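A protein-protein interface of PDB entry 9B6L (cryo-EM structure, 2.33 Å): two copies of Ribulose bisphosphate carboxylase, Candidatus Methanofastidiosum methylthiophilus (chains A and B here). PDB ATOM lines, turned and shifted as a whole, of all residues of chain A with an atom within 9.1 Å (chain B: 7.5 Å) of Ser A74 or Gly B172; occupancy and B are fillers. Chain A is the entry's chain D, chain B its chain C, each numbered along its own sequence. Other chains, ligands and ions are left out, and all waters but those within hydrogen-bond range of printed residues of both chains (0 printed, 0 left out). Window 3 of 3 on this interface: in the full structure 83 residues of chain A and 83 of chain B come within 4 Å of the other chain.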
ATOM      1  N   GLY A  19      26.720  37.004   9.352  1.00  0.00           N
ATOM      2  CA  GLY A  19      26.724  35.922   8.383  1.00  0.00           C
ATOM      3  C   GLY A  19      25.452  35.800   7.564  1.00  0.00           C
ATOM      4  O   GLY A  19      25.460  35.101   6.545  1.00  0.00           O
ATOM      5  N   TYR A  20      24.364  36.449   7.981  1.00  0.00           N
ATOM      6  CA  TYR A  20      23.089  36.367   7.280  1.00  0.00           C
ATOM      7  C   TYR A  20      22.697  37.674   6.607  1.00  0.00           C
ATOM      8  O   TYR A  20      21.573  37.789   6.109  1.00  0.00           O
ATOM      9  CB  TYR A  20      21.988  35.918   8.244  1.00  0.00           C
ATOM     10  CG  TYR A  20      22.149  34.487   8.684  1.00  0.00           C
ATOM     11  CD1 TYR A  20      21.707  33.443   7.884  1.00  0.00           C
ATOM     12  CD2 TYR A  20      22.776  34.175   9.880  1.00  0.00           C
ATOM     13  CE1 TYR A  20      21.863  32.132   8.277  1.00  0.00           C
ATOM     14  CE2 TYR A  20      22.940  32.867  10.277  1.00  0.00           C
ATOM     15  CZ  TYR A  20      22.484  31.851   9.473  1.00  0.00           C
ATOM     16  OH  TYR A  20      22.644  30.547   9.871  1.00  0.00           O
ATOM     17  N   ALA A  57      18.327  33.673   9.534  1.00  0.00           N
ATOM     18  CA  ALA A  57      18.933  32.508  10.167  1.00  0.00           C
ATOM     19  C   ALA A  57      17.889  31.441  10.466  1.00  0.00           C
ATOM     20  O   ALA A  57      18.052  30.274  10.093  1.00  0.00           O
ATOM     21  CB  ALA A  57      19.661  32.925  11.444  1.00  0.00           C
ATOM     22  N   SER A  60      16.699  29.731   7.237  1.00  0.00           N
ATOM     23  CA  SER A  60      17.590  28.912   6.419  1.00  0.00           C
ATOM     24  C   SER A  60      18.389  27.892   7.220  1.00  0.00           C
ATOM     25  O   SER A  60      18.199  26.687   7.037  1.00  0.00           O
ATOM     26  CB  SER A  60      18.547  29.811   5.632  1.00  0.00           C
ATOM     27  OG  SER A  60      19.333  30.600   6.505  1.00  0.00           O
ATOM     28  N   THR A  61      19.262  28.339   8.124  1.00  0.00           N
ATOM     29  CA  THR A  61      20.226  27.446   8.758  1.00  0.00           C
ATOM     30  C   THR A  61      20.348  27.632  10.261  1.00  0.00           C
ATOM     31  O   THR A  61      20.941  26.770  10.913  1.00  0.00           O
ATOM     32  CB  THR A  61      21.625  27.603   8.130  1.00  0.00           C
ATOM     33  OG1 THR A  61      22.073  28.956   8.266  1.00  0.00           O
ATOM     34  CG2 THR A  61      21.625  27.210   6.656  1.00  0.00           C
ATOM     35  N   GLY A  62      19.833  28.718  10.828  1.00  0.00           N
ATOM     36  CA  GLY A  62      19.743  28.850  12.274  1.00  0.00           C
ATOM     37  C   GLY A  62      21.064  28.840  13.005  1.00  0.00           C
ATOM     38  O   GLY A  62      21.192  28.169  14.036  1.00  0.00           O
ATOM     39  N   THR A  63      22.056  29.565  12.500  1.00  0.00           N
ATOM     40  CA  THR A  63      23.334  29.704  13.188  1.00  0.00           C
ATOM     41  C   THR A  63      23.457  31.156  13.638  1.00  0.00           C
ATOM     42  O   THR A  63      24.105  31.981  12.996  1.00  0.00           O
ATOM     43  CB  THR A  63      24.498  29.286  12.285  1.00  0.00           C
ATOM     44  OG1 THR A  63      24.161  28.075  11.599  1.00  0.00           O
ATOM     45  CG2 THR A  63      25.748  29.050  13.112  1.00  0.00           C
ATOM     46  N   VAL A  67      28.803  27.842  17.304  1.00  0.00           N
ATOM     47  CA  VAL A  67      28.774  26.389  17.412  1.00  0.00           C
ATOM     48  C   VAL A  67      29.981  25.828  16.674  1.00  0.00           C
ATOM     49  O   VAL A  67      30.348  26.318  15.600  1.00  0.00           O
ATOM     50  CB  VAL A  67      27.460  25.792  16.860  1.00  0.00           C
ATOM     51  CG1 VAL A  67      26.283  26.224  17.716  1.00  0.00           C
ATOM     52  CG2 VAL A  67      27.240  26.196  15.410  1.00  0.00           C
ATOM     53  N   ASN A  68      30.608  24.809  17.260  1.00  0.00           N
ATOM     54  CA  ASN A  68      31.755  24.173  16.626  1.00  0.00           C
ATOM     55  C   ASN A  68      31.361  23.270  15.466  1.00  0.00           C
ATOM     56  O   ASN A  68      32.245  22.795  14.745  1.00  0.00           O
ATOM     57  CB  ASN A  68      32.556  23.373  17.655  1.00  0.00           C
ATOM     58  CG  ASN A  68      31.723  22.315  18.348  1.00  0.00           C
ATOM     59  OD1 ASN A  68      30.509  22.459  18.492  1.00  0.00           O
ATOM     60  ND2 ASN A  68      32.373  21.241  18.780  1.00  0.00           N
ATOM     61  N   THR A  69      30.068  23.026  15.268  1.00  0.00           N
ATOM     62  CA  THR A  69      29.582  22.217  14.161  1.00  0.00           C
ATOM     63  C   THR A  69      29.342  23.031  12.897  1.00  0.00           C
ATOM     64  O   THR A  69      28.940  22.462  11.879  1.00  0.00           O
ATOM     65  CB  THR A  69      28.287  21.500  14.557  1.00  0.00           C
ATOM     66  OG1 THR A  69      27.514  22.348  15.414  1.00  0.00           O
ATOM     67  CG2 THR A  69      28.598  20.205  15.286  1.00  0.00           C
ATOM     68  N   GLU A  70      29.572  24.341  12.941  1.00  0.00           N
ATOM     69  CA  GLU A  70      29.411  25.173  11.758  1.00  0.00           C
ATOM     70  C   GLU A  70      30.459  24.820  10.710  1.00  0.00           C
ATOM     71  O   GLU A  70      31.641  24.652  11.020  1.00  0.00           O
ATOM     72  CB  GLU A  70      29.516  26.651  12.134  1.00  0.00           C
ATOM     73  CG  GLU A  70      28.769  27.591  11.200  1.00  0.00           C
ATOM     74  CD  GLU A  70      29.272  29.019  11.294  1.00  0.00           C
ATOM     75  OE1 GLU A  70      30.412  29.279  10.860  1.00  0.00           O
ATOM     76  OE2 GLU A  70      28.527  29.886  11.797  1.00  0.00           O
ATOM     77  N   THR A  71      30.016  24.707   9.460  1.00  0.00           N
ATOM     78  CA  THR A  71      30.878  24.376   8.339  1.00  0.00           C
ATOM     79  C   THR A  71      30.788  25.463   7.275  1.00  0.00           C
ATOM     80  O   THR A  71      29.787  26.182   7.205  1.00  0.00           O
ATOM     81  CB  THR A  71      30.494  23.025   7.721  1.00  0.00           C
ATOM     82  OG1 THR A  71      29.241  23.146   7.039  1.00  0.00           O
ATOM     83  CG2 THR A  71      30.374  21.960   8.797  1.00  0.00           C
ATOM     84  N   PRO A  72      31.825  25.627   6.447  1.00  0.00           N
ATOM     85  CA  PRO A  72      31.738  26.619   5.362  1.00  0.00           C
ATOM     86  C   PRO A  72      30.606  26.351   4.385  1.00  0.00           C
ATOM     87  O   PRO A  72      30.036  27.304   3.837  1.00  0.00           O
ATOM     88  CB  PRO A  72      33.112  26.523   4.682  1.00  0.00           C
ATOM     89  CG  PRO A  72      33.713  25.241   5.164  1.00  0.00           C
ATOM     90  CD  PRO A  72      33.162  25.019   6.531  1.00  0.00           C
ATOM     91  N   PHE A  73      30.255  25.086   4.149  1.00  0.00           N
ATOM     92  CA  PHE A  73      29.147  24.790   3.246  1.00  0.00           C
ATOM     93  C   PHE A  73      27.814  25.224   3.846  1.00  0.00           C
ATOM     94  O   PHE A  73      26.955  25.774   3.141  1.00  0.00           O
ATOM     95  CB  PHE A  73      29.130  23.301   2.907  1.00  0.00           C
ATOM     96  CG  PHE A  73      28.144  22.943   1.841  1.00  0.00           C
ATOM     97  CD1 PHE A  73      28.469  23.090   0.504  1.00  0.00           C
ATOM     98  CD2 PHE A  73      26.886  22.481   2.174  1.00  0.00           C
ATOM     99  CE1 PHE A  73      27.561  22.770  -0.480  1.00  0.00           C
ATOM    100  CE2 PHE A  73      25.976  22.167   1.198  1.00  0.00           C
ATOM    101  CZ  PHE A  73      26.312  22.305  -0.133  1.00  0.00           C
ATOM    102  N   SER A  74      27.621  24.990   5.147  1.00  0.00           N
ATOM    103  CA  SER A  74      26.416  25.480   5.804  1.00  0.00           C
ATOM    104  C   SER A  74      26.368  27.002   5.795  1.00  0.00           C
ATOM    105  O   SER A  74      25.284  27.589   5.736  1.00  0.00           O
ATOM    106  CB  SER A  74      26.333  24.941   7.234  1.00  0.00           C
ATOM    107  OG  SER A  74      27.255  25.588   8.089  1.00  0.00           O
ATOM    108  N   LYS A  75      27.531  27.656   5.846  1.00  0.00           N
ATOM    109  CA  LYS A  75      27.571  29.102   5.655  1.00  0.00           C
ATOM    110  C   LYS A  75      27.142  29.476   4.243  1.00  0.00           C
ATOM    111  O   LYS A  75      26.493  30.507   4.036  1.00  0.00           O
ATOM    112  CB  LYS A  75      28.971  29.639   5.944  1.00  0.00           C
ATOM    113  CG  LYS A  75      29.116  30.312   7.292  1.00  0.00           C
ATOM    114  CD  LYS A  75      30.572  30.615   7.600  1.00  0.00           C
ATOM    115  CE  LYS A  75      31.365  29.340   7.825  1.00  0.00           C
ATOM    116  NZ  LYS A  75      32.791  29.493   7.427  1.00  0.00           N
ATOM    117  N   GLU A  76      27.516  28.660   3.255  1.00  0.00           N
ATOM    118  CA  GLU A  76      27.057  28.902   1.891  1.00  0.00           C
ATOM    119  C   GLU A  76      25.542  28.787   1.786  1.00  0.00           C
ATOM    120  O   GLU A  76      24.918  29.518   1.010  1.00  0.00           O
ATOM    121  CB  GLU A  76      27.730  27.928   0.922  1.00  0.00           C
ATOM    122  CG  GLU A  76      29.239  28.074   0.819  1.00  0.00           C
ATOM    123  CD  GLU A  76      29.688  29.517   0.704  1.00  0.00           C
ATOM    124  OE1 GLU A  76      29.150  30.247  -0.153  1.00  0.00           O
ATOM    125  OE2 GLU A  76      30.585  29.919   1.472  1.00  0.00           O
ATOM    126  N   MET A  77      24.934  27.888   2.558  1.00  0.00           N
ATOM    127  CA  MET A  77      23.483  27.727   2.520  1.00  0.00           C
ATOM    128  C   MET A  77      22.722  28.801   3.295  1.00  0.00           C
ATOM    129  O   MET A  77      21.498  28.692   3.416  1.00  0.00           O
ATOM    130  CB  MET A  77      23.090  26.343   3.048  1.00  0.00           C
ATOM    131  CG  MET A  77      23.599  25.189   2.205  1.00  0.00           C
ATOM    132  SD  MET A  77      22.852  25.158   0.565  1.00  0.00           S
ATOM    133  CE  MET A  77      24.253  25.598  -0.454  1.00  0.00           C
ATOM    134  N   ASN A  78      23.398  29.821   3.818  1.00  0.00           N
ATOM    135  CA  ASN A  78      22.721  30.863   4.585  1.00  0.00           C
ATOM    136  C   ASN A  78      21.786  31.689   3.709  1.00  0.00           C
ATOM    137  O   ASN A  78      22.127  32.062   2.584  1.00  0.00           O
ATOM    138  CB  ASN A  78      23.743  31.796   5.236  1.00  0.00           C
ATOM    139  CG  ASN A  78      24.400  31.191   6.453  1.00  0.00           C
ATOM    140  OD1 ASN A  78      24.158  30.037   6.796  1.00  0.00           O
ATOM    141  ND2 ASN A  78      25.232  31.975   7.120  1.00  0.00           N
ATOM    142  N   ALA A  79      20.601  31.987   4.239  1.00  0.00           N
ATOM    143  CA  ALA A  79      19.767  33.028   3.658  1.00  0.00           C
ATOM    144  C   ALA A  79      20.377  34.388   3.959  1.00  0.00           C
ATOM    145  O   ALA A  79      20.873  34.632   5.060  1.00  0.00           O
ATOM    146  CB  ALA A  79      18.343  32.955   4.202  1.00  0.00           C
ATOM    147  N   PRO A  96      18.970  30.519  -0.838  1.00  0.00           N
ATOM    148  CA  PRO A  96      19.493  29.522  -1.780  1.00  0.00           C
ATOM    149  C   PRO A  96      18.537  28.348  -1.893  1.00  0.00           C
ATOM    150  O   PRO A  96      18.308  27.648  -0.905  1.00  0.00           O
ATOM    151  CB  PRO A  96      20.832  29.105  -1.155  1.00  0.00           C
ATOM    152  CG  PRO A  96      21.193  30.214  -0.227  1.00  0.00           C
ATOM    153  CD  PRO A  96      19.904  30.789   0.267  1.00  0.00           C
ATOM    154  N   ARG A  98      18.759  25.510  -2.921  1.00  0.00           N
ATOM    155  CA  ARG A  98      19.282  24.209  -2.529  1.00  0.00           C
ATOM    156  C   ARG A  98      18.802  23.799  -1.145  1.00  0.00           C
ATOM    157  O   ARG A  98      18.807  22.606  -0.824  1.00  0.00           O
ATOM    158  CB  ARG A  98      20.808  24.227  -2.564  1.00  0.00           C
ATOM    159  CG  ARG A  98      21.398  24.052  -3.944  1.00  0.00           C
ATOM    160  CD  ARG A  98      22.906  24.157  -3.894  1.00  0.00           C
ATOM    161  NE  ARG A  98      23.538  22.854  -3.732  1.00  0.00           N
ATOM    162  CZ  ARG A  98      24.844  22.644  -3.801  1.00  0.00           C
ATOM    163  NH1 ARG A  98      25.691  23.635  -4.027  1.00  0.00           N
ATOM    164  NH2 ARG A  98      25.311  21.411  -3.642  1.00  0.00           N
ATOM    165  N   LEU A  99      18.391  24.766  -0.319  1.00  0.00           N
ATOM    166  CA  LEU A  99      17.831  24.459   0.993  1.00  0.00           C
ATOM    167  C   LEU A  99      16.563  23.627   0.889  1.00  0.00           C
ATOM    168  O   LEU A  99      16.266  22.834   1.787  1.00  0.00           O
ATOM    169  CB  LEU A  99      17.528  25.753   1.746  1.00  0.00           C
ATOM    170  CG  LEU A  99      18.707  26.596   2.222  1.00  0.00           C
ATOM    171  CD1 LEU A  99      18.272  28.038   2.414  1.00  0.00           C
ATOM    172  CD2 LEU A  99      19.269  26.027   3.508  1.00  0.00           C
ATOM    173  N   TYR A 112      10.163  26.586   5.471  1.00  0.00           N
ATOM    174  CA  TYR A 112      11.352  27.423   5.589  1.00  0.00           C
ATOM    175  C   TYR A 112      10.984  28.885   5.827  1.00  0.00           C
ATOM    176  O   TYR A 112      11.348  29.473   6.851  1.00  0.00           O
ATOM    177  CB  TYR A 112      12.206  27.299   4.326  1.00  0.00           C
ATOM    178  CG  TYR A 112      13.313  26.271   4.381  1.00  0.00           C
ATOM    179  CD1 TYR A 112      14.422  26.452   5.196  1.00  0.00           C
ATOM    180  CD2 TYR A 112      13.265  25.137   3.591  1.00  0.00           C
ATOM    181  CE1 TYR A 112      15.442  25.527   5.230  1.00  0.00           C
ATOM    182  CE2 TYR A 112      14.276  24.207   3.618  1.00  0.00           C
ATOM    183  CZ  TYR A 112      15.364  24.403   4.439  1.00  0.00           C
ATOM    184  OH  TYR A 112      16.371  23.471   4.465  1.00  0.00           O
ATOM    185  N   LYS B 168      22.494  22.044  15.535  1.00  0.00           N
ATOM    186  CA  LYS B 168      22.941  23.325  15.020  1.00  0.00           C
ATOM    187  C   LYS B 168      24.246  23.142  14.263  1.00  0.00           C
ATOM    188  O   LYS B 168      25.182  22.541  14.808  1.00  0.00           O
ATOM    189  CB  LYS B 168      23.132  24.333  16.157  1.00  0.00           C
ATOM    190  CG  LYS B 168      21.850  24.715  16.875  1.00  0.00           C
ATOM    191  CD  LYS B 168      20.965  25.578  15.996  1.00  0.00           C
ATOM    192  CE  LYS B 168      20.201  26.602  16.818  1.00  0.00           C
ATOM    193  NZ  LYS B 168      19.206  27.342  15.995  1.00  0.00           N
ATOM    194  N   PRO B 169      24.366  23.637  13.022  1.00  0.00           N
ATOM    195  CA  PRO B 169      23.381  24.408  12.241  1.00  0.00           C
ATOM    196  C   PRO B 169      22.131  23.612  11.876  1.00  0.00           C
ATOM    197  O   PRO B 169      22.175  22.392  11.755  1.00  0.00           O
ATOM    198  CB  PRO B 169      24.169  24.801  10.978  1.00  0.00           C
ATOM    199  CG  PRO B 169      25.611  24.718  11.373  1.00  0.00           C
ATOM    200  CD  PRO B 169      25.666  23.572  12.336  1.00  0.00           C
ATOM    201  N   LYS B 170      21.005  24.310  11.710  1.00  0.00           N
ATOM    202  CA  LYS B 170      19.755  23.656  11.331  1.00  0.00           C
ATOM    203  C   LYS B 170      19.911  22.888  10.026  1.00  0.00           C
ATOM    204  O   LYS B 170      19.467  21.740   9.908  1.00  0.00           O
ATOM    205  CB  LYS B 170      18.647  24.700  11.186  1.00  0.00           C
ATOM    206  CG  LYS B 170      17.782  24.911  12.406  1.00  0.00           C
ATOM    207  CD  LYS B 170      17.177  26.314  12.428  1.00  0.00           C
ATOM    208  CE  LYS B 170      16.945  26.887  11.030  1.00  0.00           C
ATOM    209  NZ  LYS B 170      15.937  26.139  10.231  1.00  0.00           N
ATOM    210  N   MET B 171      20.528  23.515   9.031  1.00  0.00           N
ATOM    211  CA  MET B 171      20.695  22.948   7.706  1.00  0.00           C
ATOM    212  C   MET B 171      22.099  23.250   7.207  1.00  0.00           C
ATOM    213  O   MET B 171      22.849  24.015   7.818  1.00  0.00           O
ATOM    214  CB  MET B 171      19.649  23.496   6.723  1.00  0.00           C
ATOM    215  CG  MET B 171      18.215  23.149   7.081  1.00  0.00           C
ATOM    216  SD  MET B 171      17.812  21.415   6.796  1.00  0.00           S
ATOM    217  CE  MET B 171      18.689  21.110   5.268  1.00  0.00           C
ATOM    218  N   GLY B 172      22.449  22.640   6.081  1.00  0.00           N
ATOM    219  CA  GLY B 172      23.763  22.803   5.501  1.00  0.00           C
ATOM    220  C   GLY B 172      24.791  21.791   5.948  1.00  0.00           C
ATOM    221  O   GLY B 172      25.926  21.829   5.458  1.00  0.00           O
ATOM    222  N   LEU B 173      24.439  20.896   6.863  1.00  0.00           N
ATOM    223  CA  LEU B 173      25.329  19.820   7.265  1.00  0.00           C
ATOM    224  C   LEU B 173      25.128  18.614   6.360  1.00  0.00           C
ATOM    225  O   LEU B 173      24.044  18.392   5.816  1.00  0.00           O
ATOM    226  CB  LEU B 173      25.082  19.418   8.721  1.00  0.00           C
ATOM    227  CG  LEU B 173      25.451  20.422   9.814  1.00  0.00           C
ATOM    228  CD1 LEU B 173      25.281  19.793  11.184  1.00  0.00           C
ATOM    229  CD2 LEU B 173      26.869  20.927   9.628  1.00  0.00           C
ATOM    230  N   THR B 174      26.191  17.838   6.197  1.00  0.00           N
ATOM    231  CA  THR B 174      26.077  16.580   5.484  1.00  0.00           C
ATOM    232  C   THR B 174      25.401  15.540   6.372  1.00  0.00           C
ATOM    233  O   THR B 174      25.229  15.731   7.578  1.00  0.00           O
ATOM    234  CB  THR B 174      27.452  16.090   5.033  1.00  0.00           C
ATOM    235  OG1 THR B 174      28.220  15.688   6.172  1.00  0.00           O
ATOM    236  CG2 THR B 174      28.194  17.182   4.277  1.00  0.00           C
ATOM    237  N   SER B 175      24.999  14.427   5.756  1.00  0.00           N
ATOM    238  CA  SER B 175      24.413  13.336   6.527  1.00  0.00           C
ATOM    239  C   SER B 175      25.364  12.871   7.618  1.00  0.00           C
ATOM    240  O   SER B 175      24.946  12.627   8.755  1.00  0.00           O
ATOM    241  CB  SER B 175      24.049  12.175   5.605  1.00  0.00           C
ATOM    242  OG  SER B 175      23.493  12.641   4.391  1.00  0.00           O
ATOM    243  N   GLU B 177      27.860  14.659   9.022  1.00  0.00           N
ATOM    244  CA  GLU B 177      28.001  15.700  10.038  1.00  0.00           C
ATOM    245  C   GLU B 177      26.789  15.738  10.961  1.00  0.00           C
ATOM    246  O   GLU B 177      26.930  15.839  12.188  1.00  0.00           O
ATOM    247  CB  GLU B 177      28.205  17.058   9.369  1.00  0.00           C
ATOM    248  CG  GLU B 177      29.654  17.392   9.060  1.00  0.00           C
ATOM    249  CD  GLU B 177      29.803  18.194   7.782  1.00  0.00           C
ATOM    250  OE1 GLU B 177      28.771  18.532   7.168  1.00  0.00           O
ATOM    251  OE2 GLU B 177      30.953  18.491   7.392  1.00  0.00           O
ATOM    252  N   GLN B 199      14.123  19.732   7.268  1.00  0.00           N
ATOM    253  CA  GLN B 199      15.181  18.809   6.877  1.00  0.00           C
ATOM    254  C   GLN B 199      14.577  17.617   6.147  1.00  0.00           C
ATOM    255  O   GLN B 199      13.769  16.875   6.712  1.00  0.00           O
ATOM    256  CB  GLN B 199      15.971  18.352   8.100  1.00  0.00           C
ATOM    257  CG  GLN B 199      16.959  17.231   7.823  1.00  0.00           C
ATOM    258  CD  GLN B 199      18.037  17.138   8.881  1.00  0.00           C
ATOM    259  OE1 GLN B 199      17.896  17.679   9.976  1.00  0.00           O
ATOM    260  NE2 GLN B 199      19.123  16.448   8.557  1.00  0.00           N
ATOM    261  N   GLN B 202      17.410  16.920   0.830  1.00  0.00           N
ATOM    262  CA  GLN B 202      18.226  17.944   0.197  1.00  0.00           C
ATOM    263  C   GLN B 202      19.401  17.301  -0.530  1.00  0.00           C
ATOM    264  O   GLN B 202      19.857  16.212  -0.175  1.00  0.00           O
ATOM    265  CB  GLN B 202      18.739  18.951   1.229  1.00  0.00           C
ATOM    266  CG  GLN B 202      17.775  20.084   1.534  1.00  0.00           C
ATOM    267  CD  GLN B 202      16.805  19.752   2.650  1.00  0.00           C
ATOM    268  OE1 GLN B 202      17.062  18.868   3.462  1.00  0.00           O
ATOM    269  NE2 GLN B 202      15.689  20.466   2.700  1.00  0.00           N
ATOM    270  N   PHE B 204      22.587  18.111  -0.737  1.00  0.00           N
ATOM    271  CA  PHE B 204      23.810  17.975   0.041  1.00  0.00           C
ATOM    272  C   PHE B 204      23.652  17.066   1.251  1.00  0.00           C
ATOM    273  O   PHE B 204      24.661  16.660   1.839  1.00  0.00           O
ATOM    274  CB  PHE B 204      24.292  19.349   0.512  1.00  0.00           C
ATOM    275  CG  PHE B 204      23.220  20.186   1.151  1.00  0.00           C
ATOM    276  CD1 PHE B 204      22.923  20.047   2.497  1.00  0.00           C
ATOM    277  CD2 PHE B 204      22.516  21.119   0.409  1.00  0.00           C
ATOM    278  CE1 PHE B 204      21.938  20.814   3.087  1.00  0.00           C
ATOM    279  CE2 PHE B 204      21.532  21.891   0.995  1.00  0.00           C
ATOM    280  CZ  PHE B 204      21.243  21.739   2.336  1.00  0.00           C
ATOM    281  N   CYS B 205      22.422  16.760   1.648  1.00  0.00           N
ATOM    282  CA  CYS B 205      22.139  15.845   2.753  1.00  0.00           C
ATOM    283  C   CYS B 205      21.015  14.915   2.320  1.00  0.00           C
ATOM    284  O   CYS B 205      19.865  15.066   2.750  1.00  0.00           O
ATOM    285  CB  CYS B 205      21.773  16.613   4.024  1.00  0.00           C
ATOM    286  SG  CYS B 205      21.787  15.633   5.544  1.00  0.00           S
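The backbone carbonyl oxygen (O) of Thr A61 lies within hydrogen-bond range of the backbone NH (N) of Lys B170.
The backbone carbonyl oxygen of Lys B168 lies within hydrogen-bond range of the side-chain hydroxyl of Thr A69 (2.4 Å).
The side-chain amino group (NZ) of Lys B168 sits at hydrogen-bond distance from the backbone carbonyl oxygen (O) of Gly A62 (2.9 Å).
The side-chain sulfur (SD) of Met B171 lies close to the side-chain hydroxyl (OH) of Tyr A112 (3.4 Å).
The side-chain amide nitrogen (NE2) of Gln B202 is in hydrogen-bond range of the backbone carbonyl oxygen (O) of Leu A99.
SG of Cys B205 sits close to O of Leu B173, at 3.6 Å.
The backbone carbonyl oxygen (O) of Ser A74 lies close to the side-chain amide oxygen (OD1) of Asn A78 (2.9 Å).
The side-chain hydroxyl (OH) of Tyr A20 sits at hydrogen-bond distance from the backbone NH (N) of Thr A63.
OH of Tyr A20 sits at hydrogen-bond distance from N of Gly A62 (3.5 Å).
The side-chain hydroxyl of Ser A74 sits at hydrogen-bond distance from the backbone carbonyl oxygen of Thr A71 (2.7 Å).
The side-chain hydroxyl (OG) of Ser A60 sits at hydrogen-bond distance from the backbone NH (N) of Ala A79 (2.9 Å).
NZ of Lys B170 touches O of Ser A60, 3.95 Å away.
Met B171 touches Ser A60.
CG2 of Thr A61 touches O of Met B171 (3.6 Å).
Thr A63 touches Pro B169.
Glu A70 touches Pro B169 (CA to CG, 3.8 Å).
CD2 of Phe A73 touches O of Gly B172, 3.5 Å away.
CB of Phe B204 touches CE2 of Phe A73, at 3.4 Å.
Met A77 touches Phe B204 (SD to CE2, 3.5 Å).
O of Arg A98 touches CE2 of Phe B204, at 3.4 Å.
NE2 of Gln B202 touches OH of Tyr A112, at 3.6 Å.
Printed residues of chain B within 4 Å of Phe A73: Gly B172 and Phe B204.
Of the printed residues of chain B, Arg A98 touches Gln B202 (3.6 Å) and Phe B204 (3.4 Å).
Printed residues of chain A within 4 Å of Pro B169: Thr A61, Thr A63, Thr A69, Glu A70 and Ser A74.
Gly B172 touches three residues of chain A.
Gln B199 touches none of the printed residues of chain A.
The nearest residue of chain A that does not touch Gly B172 is Met A77 (4.1 Å).
Hydrophobic or aromatic side chains of chain A that line the printed part of chain B: Val A67, Phe A73, Met A77 and Tyr A112.
Of the 13 printed residues of chain B, 9 touch a printed residue of chain A.
Hydrophobic or aromatic side chains of chain B that line the printed part of chain A: Pro B169, Met B171, Leu B173 and Phe B204.
Along chain B the printed residues that touch a printed residue of chain A span positions 168 to 204.
Among the printed residues, 28 pairs touch across the chains.
No position is printed for both chains.
Of the 28 pairs that touch across the chains among the printed residues, none has its exchanged pair printed and touching as well.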
